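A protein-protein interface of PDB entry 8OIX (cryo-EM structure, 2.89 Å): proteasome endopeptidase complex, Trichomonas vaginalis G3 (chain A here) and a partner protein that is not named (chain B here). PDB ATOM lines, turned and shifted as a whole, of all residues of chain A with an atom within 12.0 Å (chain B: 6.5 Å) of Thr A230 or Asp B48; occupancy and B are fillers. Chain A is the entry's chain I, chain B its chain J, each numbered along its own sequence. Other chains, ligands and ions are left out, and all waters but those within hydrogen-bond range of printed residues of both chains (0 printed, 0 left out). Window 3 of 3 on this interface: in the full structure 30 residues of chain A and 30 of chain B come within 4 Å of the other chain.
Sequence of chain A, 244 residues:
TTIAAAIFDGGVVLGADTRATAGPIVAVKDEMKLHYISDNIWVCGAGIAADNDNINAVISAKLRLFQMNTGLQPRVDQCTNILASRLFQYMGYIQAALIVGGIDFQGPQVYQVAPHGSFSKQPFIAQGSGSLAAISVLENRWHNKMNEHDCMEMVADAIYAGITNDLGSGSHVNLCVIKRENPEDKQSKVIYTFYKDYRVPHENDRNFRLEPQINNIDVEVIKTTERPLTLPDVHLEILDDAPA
The backbone NH (N) of Val B196 is in hydrogen-bond range of the backbone carbonyl oxygen (O) of Arg A227 (2.5 Å). O of Asp B194 is in hydrogen-bond range of N of Leu A229.
Of chain B, only Asp B48 comes within 4 Å of Thr A230. Asp B48 touches two residues of chain A. No residue of chain A comes within 4 Å of Asn B47. Of the printed residues of chain B, Leu A229 touches Asp B48, Arg B49, Ile B191, Thr B192, Asp B194 and Val B196. Printed residues of chain A within 4 Å of Asp B194: Pro A228 (3.7 Å) and Leu A229 (2.9 Å). Gln B45 touches none of the printed residues of chain A. The nearest residue of chain B that does not touch Thr A230 is Asp B194 (5.2 Å). The nearest printed residue of chain B that does not touch Leu A229 is Tyr B51 (5.7 Å).
OG1 of Thr A225 sits at hydrogen-bond distance from NH1 of Arg A227 (3.3 Å).
Of the 13 printed residues of chain B, 6 touch a printed residue of chain A. Hydrophobic or aromatic side chains of chain B within 4 Å of the printed part of chain A: Ile B191 and Val B196. Hydrophobic or aromatic side chains of chain A that line the printed part of chain B: Leu A229. Along chain A the printed residues that touch a printed residue of chain B span positions 225 to 230.
Among the printed residues, merely in contact across the chains: Leu A229 with Asp B48 (3.1 Å), Leu A229 with Thr B192 (3.2 Å), Glu A226 with Val B196 (3.2 Å), Leu A229 with Arg B49 (3.3 Å), Leu A229 with Ile B191 (3.5 Å), Thr A225 with Val B196 (3.6 Å), Leu A229 with Val B196 (3.6 Å), Pro A228 with Asp B194 (3.7 Å) and Thr A230 with Asp B48 (3.9 Å).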
ATOM      1  N   THR A 225       4.903  30.185  -3.763  1.00  0.00           N
ATOM      2  CA  THR A 225       4.509  29.078  -2.906  1.00  0.00           C
ATOM      3  C   THR A 225       5.732  28.224  -2.610  1.00  0.00           C
ATOM      4  O   THR A 225       6.578  28.013  -3.484  1.00  0.00           O
ATOM      5  CB  THR A 225       3.393  28.228  -3.537  1.00  0.00           C
ATOM      6  OG1 THR A 225       3.099  27.109  -2.690  1.00  0.00           O
ATOM      7  CG2 THR A 225       3.795  27.732  -4.913  1.00  0.00           C
ATOM      8  N   GLU A 226       5.830  27.753  -1.371  1.00  0.00           N
ATOM      9  CA  GLU A 226       6.915  26.886  -0.936  1.00  0.00           C
ATOM     10  C   GLU A 226       6.366  25.497  -0.649  1.00  0.00           C
ATOM     11  O   GLU A 226       5.389  25.352   0.092  1.00  0.00           O
ATOM     12  CB  GLU A 226       7.607  27.448   0.307  1.00  0.00           C
ATOM     13  CG  GLU A 226       8.114  28.868   0.147  1.00  0.00           C
ATOM     14  CD  GLU A 226       8.510  29.492   1.468  1.00  0.00           C
ATOM     15  OE1 GLU A 226       8.875  28.740   2.396  1.00  0.00           O
ATOM     16  OE2 GLU A 226       8.457  30.735   1.581  1.00  0.00           O
ATOM     17  N   ARG A 227       6.996  24.481  -1.234  1.00  0.00           N
ATOM     18  CA  ARG A 227       6.572  23.105  -1.047  1.00  0.00           C
ATOM     19  C   ARG A 227       7.747  22.267  -0.560  1.00  0.00           C
ATOM     20  O   ARG A 227       8.875  22.441  -1.038  1.00  0.00           O
ATOM     21  CB  ARG A 227       6.015  22.528  -2.358  1.00  0.00           C
ATOM     22  CG  ARG A 227       5.224  21.237  -2.205  1.00  0.00           C
ATOM     23  CD  ARG A 227       3.884  21.475  -1.519  1.00  0.00           C
ATOM     24  NE  ARG A 227       2.941  22.193  -2.369  1.00  0.00           N
ATOM     25  CZ  ARG A 227       2.566  23.451  -2.180  1.00  0.00           C
ATOM     26  NH1 ARG A 227       3.038  24.170  -1.175  1.00  0.00           N
ATOM     27  NH2 ARG A 227       1.694  24.001  -3.020  1.00  0.00           N
ATOM     28  N   PRO A 228       7.519  21.360   0.390  1.00  0.00           N
ATOM     29  CA  PRO A 228       8.619  20.535   0.903  1.00  0.00           C
ATOM     30  C   PRO A 228       9.215  19.644  -0.177  1.00  0.00           C
ATOM     31  O   PRO A 228       8.543  19.249  -1.133  1.00  0.00           O
ATOM     32  CB  PRO A 228       7.958  19.707   2.010  1.00  0.00           C
ATOM     33  CG  PRO A 228       6.775  20.510   2.423  1.00  0.00           C
ATOM     34  CD  PRO A 228       6.287  21.183   1.176  1.00  0.00           C
ATOM     35  N   LEU A 229      10.498  19.326  -0.009  1.00  0.00           N
ATOM     36  CA  LEU A 229      11.232  18.491  -0.948  1.00  0.00           C
ATOM     37  C   LEU A 229      11.064  16.999  -0.655  1.00  0.00           C
ATOM     38  O   LEU A 229      11.909  16.192  -1.058  1.00  0.00           O
ATOM     39  CB  LEU A 229      12.715  18.872  -0.925  1.00  0.00           C
ATOM     40  CG  LEU A 229      13.615  18.440  -2.083  1.00  0.00           C
ATOM     41  CD1 LEU A 229      13.604  19.508  -3.143  1.00  0.00           C
ATOM     42  CD2 LEU A 229      15.027  18.146  -1.622  1.00  0.00           C
ATOM     43  N   THR A 230       9.992  16.618   0.031  1.00  0.00           N
ATOM     44  CA  THR A 230       9.763  15.220   0.375  1.00  0.00           C
ATOM     45  C   THR A 230       8.303  14.981   0.747  1.00  0.00           C
ATOM     46  O   THR A 230       7.409  15.111  -0.090  1.00  0.00           O
ATOM     47  CB  THR A 230      10.666  14.769   1.540  1.00  0.00           C
ATOM     48  OG1 THR A 230      10.442  13.380   1.816  1.00  0.00           O
ATOM     49  CG2 THR A 230      10.376  15.585   2.789  1.00  0.00           C
ATOM     50  N   GLN B  45       7.441  18.702 -12.176  1.00  0.00           N
ATOM     51  CA  GLN B  45       8.152  18.002 -11.119  1.00  0.00           C
ATOM     52  C   GLN B  45       8.191  16.527 -11.482  1.00  0.00           C
ATOM     53  O   GLN B  45       7.143  15.894 -11.655  1.00  0.00           O
ATOM     54  CB  GLN B  45       7.474  18.213  -9.769  1.00  0.00           C
ATOM     55  CG  GLN B  45       8.188  17.531  -8.615  1.00  0.00           C
ATOM     56  CD  GLN B  45       7.466  17.702  -7.296  1.00  0.00           C
ATOM     57  OE1 GLN B  45       8.014  18.254  -6.343  1.00  0.00           O
ATOM     58  NE2 GLN B  45       6.230  17.225  -7.233  1.00  0.00           N
ATOM     59  N   ILE B  46       9.396  15.982 -11.602  1.00  0.00           N
ATOM     60  CA  ILE B  46       9.562  14.585 -11.977  1.00  0.00           C
ATOM     61  C   ILE B  46       9.790  13.790 -10.703  1.00  0.00           C
ATOM     62  O   ILE B  46       9.319  12.654 -10.565  1.00  0.00           O
ATOM     63  CB  ILE B  46      10.709  14.409 -12.988  1.00  0.00           C
ATOM     64  CG1 ILE B  46      10.178  14.484 -14.425  1.00  0.00           C
ATOM     65  CG2 ILE B  46      11.453  13.102 -12.752  1.00  0.00           C
ATOM     66  CD1 ILE B  46       9.133  15.542 -14.687  1.00  0.00           C
ATOM     67  N   ASN B  47      10.482  14.401  -9.749  1.00  0.00           N
ATOM     68  CA  ASN B  47      10.759  13.752  -8.482  1.00  0.00           C
ATOM     69  C   ASN B  47      10.856  14.843  -7.429  1.00  0.00           C
ATOM     70  O   ASN B  47      10.949  16.031  -7.752  1.00  0.00           O
ATOM     71  CB  ASN B  47      12.039  12.911  -8.561  1.00  0.00           C
ATOM     72  CG  ASN B  47      12.232  12.026  -7.353  1.00  0.00           C
ATOM     73  OD1 ASN B  47      11.381  11.196  -7.039  1.00  0.00           O
ATOM     74  ND2 ASN B  47      13.355  12.198  -6.666  1.00  0.00           N
ATOM     75  N   ASP B  48      10.886  14.423  -6.161  1.00  0.00           N
ATOM     76  CA  ASP B  48      10.963  15.383  -5.067  1.00  0.00           C
ATOM     77  C   ASP B  48      12.125  16.345  -5.247  1.00  0.00           C
ATOM     78  O   ASP B  48      12.018  17.520  -4.886  1.00  0.00           O
ATOM     79  CB  ASP B  48      11.085  14.648  -3.730  1.00  0.00           C
ATOM     80  CG  ASP B  48       9.848  13.839  -3.394  1.00  0.00           C
ATOM     81  OD1 ASP B  48       8.743  14.232  -3.824  1.00  0.00           O
ATOM     82  OD2 ASP B  48       9.980  12.814  -2.693  1.00  0.00           O
ATOM     83  N   ARG B  49      13.226  15.877  -5.829  1.00  0.00           N
ATOM     84  CA  ARG B  49      14.393  16.708  -6.081  1.00  0.00           C
ATOM     85  C   ARG B  49      14.762  16.717  -7.561  1.00  0.00           C
ATOM     86  O   ARG B  49      15.933  16.865  -7.909  1.00  0.00           O
ATOM     87  CB  ARG B  49      15.575  16.240  -5.235  1.00  0.00           C
ATOM     88  CG  ARG B  49      15.867  14.754  -5.371  1.00  0.00           C
ATOM     89  CD  ARG B  49      17.028  14.298  -4.497  1.00  0.00           C
ATOM     90  NE  ARG B  49      16.906  14.744  -3.114  1.00  0.00           N
ATOM     91  CZ  ARG B  49      17.682  15.657  -2.551  1.00  0.00           C
ATOM     92  NH1 ARG B  49      18.667  16.236  -3.218  1.00  0.00           N
ATOM     93  NH2 ARG B  49      17.474  15.992  -1.281  1.00  0.00           N
ATOM     94  N   ILE B  50      13.779  16.552  -8.448  1.00  0.00           N
ATOM     95  CA  ILE B  50      14.011  16.633  -9.888  1.00  0.00           C
ATOM     96  C   ILE B  50      12.859  17.387 -10.531  1.00  0.00           C
ATOM     97  O   ILE B  50      11.696  17.007 -10.358  1.00  0.00           O
ATOM     98  CB  ILE B  50      14.144  15.245 -10.545  1.00  0.00           C
ATOM     99  CG1 ILE B  50      15.261  14.427  -9.907  1.00  0.00           C
ATOM    100  CG2 ILE B  50      14.388  15.387 -12.037  1.00  0.00           C
ATOM    101  CD1 ILE B  50      15.333  13.026 -10.442  1.00  0.00           C
ATOM    102  N   TYR B  51      13.184  18.413 -11.319  1.00  0.00           N
ATOM    103  CA  TYR B  51      12.214  19.143 -12.119  1.00  0.00           C
ATOM    104  C   TYR B  51      12.662  19.139 -13.572  1.00  0.00           C
ATOM    105  O   TYR B  51      13.850  19.296 -13.867  1.00  0.00           O
ATOM    106  CB  TYR B  51      12.046  20.577 -11.614  1.00  0.00           C
ATOM    107  CG  TYR B  51      11.161  20.672 -10.395  1.00  0.00           C
ATOM    108  CD1 TYR B  51      11.597  20.215  -9.160  1.00  0.00           C
ATOM    109  CD2 TYR B  51       9.885  21.206 -10.482  1.00  0.00           C
ATOM    110  CE1 TYR B  51      10.790  20.292  -8.046  1.00  0.00           C
ATOM    111  CE2 TYR B  51       9.071  21.286  -9.373  1.00  0.00           C
ATOM    112  CZ  TYR B  51       9.528  20.829  -8.158  1.00  0.00           C
ATOM    113  OH  TYR B  51       8.716  20.910  -7.051  1.00  0.00           O
ATOM    114  N   GLU B  76      10.044   3.771 -10.246  1.00  0.00           N
ATOM    115  CA  GLU B  76       9.914   3.925  -8.803  1.00  0.00           C
ATOM    116  C   GLU B  76       9.024   2.849  -8.199  1.00  0.00           C
ATOM    117  O   GLU B  76       9.206   2.483  -7.034  1.00  0.00           O
ATOM    118  CB  GLU B  76       9.378   5.315  -8.464  1.00  0.00           C
ATOM    119  CG  GLU B  76      10.315   6.446  -8.851  1.00  0.00           C
ATOM    120  CD  GLU B  76       9.709   7.810  -8.610  1.00  0.00           C
ATOM    121  OE1 GLU B  76       8.594   7.874  -8.050  1.00  0.00           O
ATOM    122  OE2 GLU B  76      10.353   8.818  -8.963  1.00  0.00           O
ATOM    123  N   PRO B  82      12.977   6.593  -5.334  1.00  0.00           N
ATOM    124  CA  PRO B  82      12.893   7.700  -6.291  1.00  0.00           C
ATOM    125  C   PRO B  82      14.045   7.655  -7.283  1.00  0.00           C
ATOM    126  O   PRO B  82      15.133   7.159  -6.985  1.00  0.00           O
ATOM    127  CB  PRO B  82      12.965   8.947  -5.402  1.00  0.00           C
ATOM    128  CG  PRO B  82      12.571   8.477  -4.045  1.00  0.00           C
ATOM    129  CD  PRO B  82      13.059   7.070  -3.944  1.00  0.00           C
ATOM    130  N   ILE B 191      14.744  24.848  -6.272  1.00  0.00           N
ATOM    131  CA  ILE B 191      14.840  23.565  -5.592  1.00  0.00           C
ATOM    132  C   ILE B 191      16.026  23.640  -4.644  1.00  0.00           C
ATOM    133  O   ILE B 191      17.157  23.913  -5.066  1.00  0.00           O
ATOM    134  CB  ILE B 191      14.994  22.409  -6.594  1.00  0.00           C
ATOM    135  CG1 ILE B 191      13.852  22.412  -7.613  1.00  0.00           C
ATOM    136  CG2 ILE B 191      15.075  21.083  -5.878  1.00  0.00           C
ATOM    137  CD1 ILE B 191      14.160  23.147  -8.899  1.00  0.00           C
ATOM    138  N   THR B 192      15.765  23.401  -3.361  1.00  0.00           N
ATOM    139  CA  THR B 192      16.773  23.442  -2.313  1.00  0.00           C
ATOM    140  C   THR B 192      16.735  22.130  -1.540  1.00  0.00           C
ATOM    141  O   THR B 192      15.988  21.208  -1.876  1.00  0.00           O
ATOM    142  CB  THR B 192      16.548  24.630  -1.371  1.00  0.00           C
ATOM    143  OG1 THR B 192      15.254  24.524  -0.767  1.00  0.00           O
ATOM    144  CG2 THR B 192      16.628  25.936  -2.138  1.00  0.00           C
ATOM    145  N   ASP B 194      15.607  21.686   1.495  1.00  0.00           N
ATOM    146  CA  ASP B 194      14.407  21.567   2.314  1.00  0.00           C
ATOM    147  C   ASP B 194      13.116  21.802   1.537  1.00  0.00           C
ATOM    148  O   ASP B 194      12.164  21.032   1.677  1.00  0.00           O
ATOM    149  CB  ASP B 194      14.484  22.543   3.494  1.00  0.00           C
ATOM    150  CG  ASP B 194      15.515  22.130   4.523  1.00  0.00           C
ATOM    151  OD1 ASP B 194      15.539  20.938   4.898  1.00  0.00           O
ATOM    152  OD2 ASP B 194      16.304  22.994   4.958  1.00  0.00           O
ATOM    153  N   VAL B 196      10.890  23.526  -2.100  1.00  0.00           N
ATOM    154  CA  VAL B 196      10.808  24.024  -3.467  1.00  0.00           C
ATOM    155  C   VAL B 196       9.965  25.290  -3.438  1.00  0.00           C
ATOM    156  O   VAL B 196       8.810  25.266  -2.997  1.00  0.00           O
ATOM    157  CB  VAL B 196      10.207  22.984  -4.424  1.00  0.00           C
ATOM    158  CG1 VAL B 196      10.144  23.545  -5.834  1.00  0.00           C
ATOM    159  CG2 VAL B 196      11.019  21.705  -4.393  1.00  0.00           C
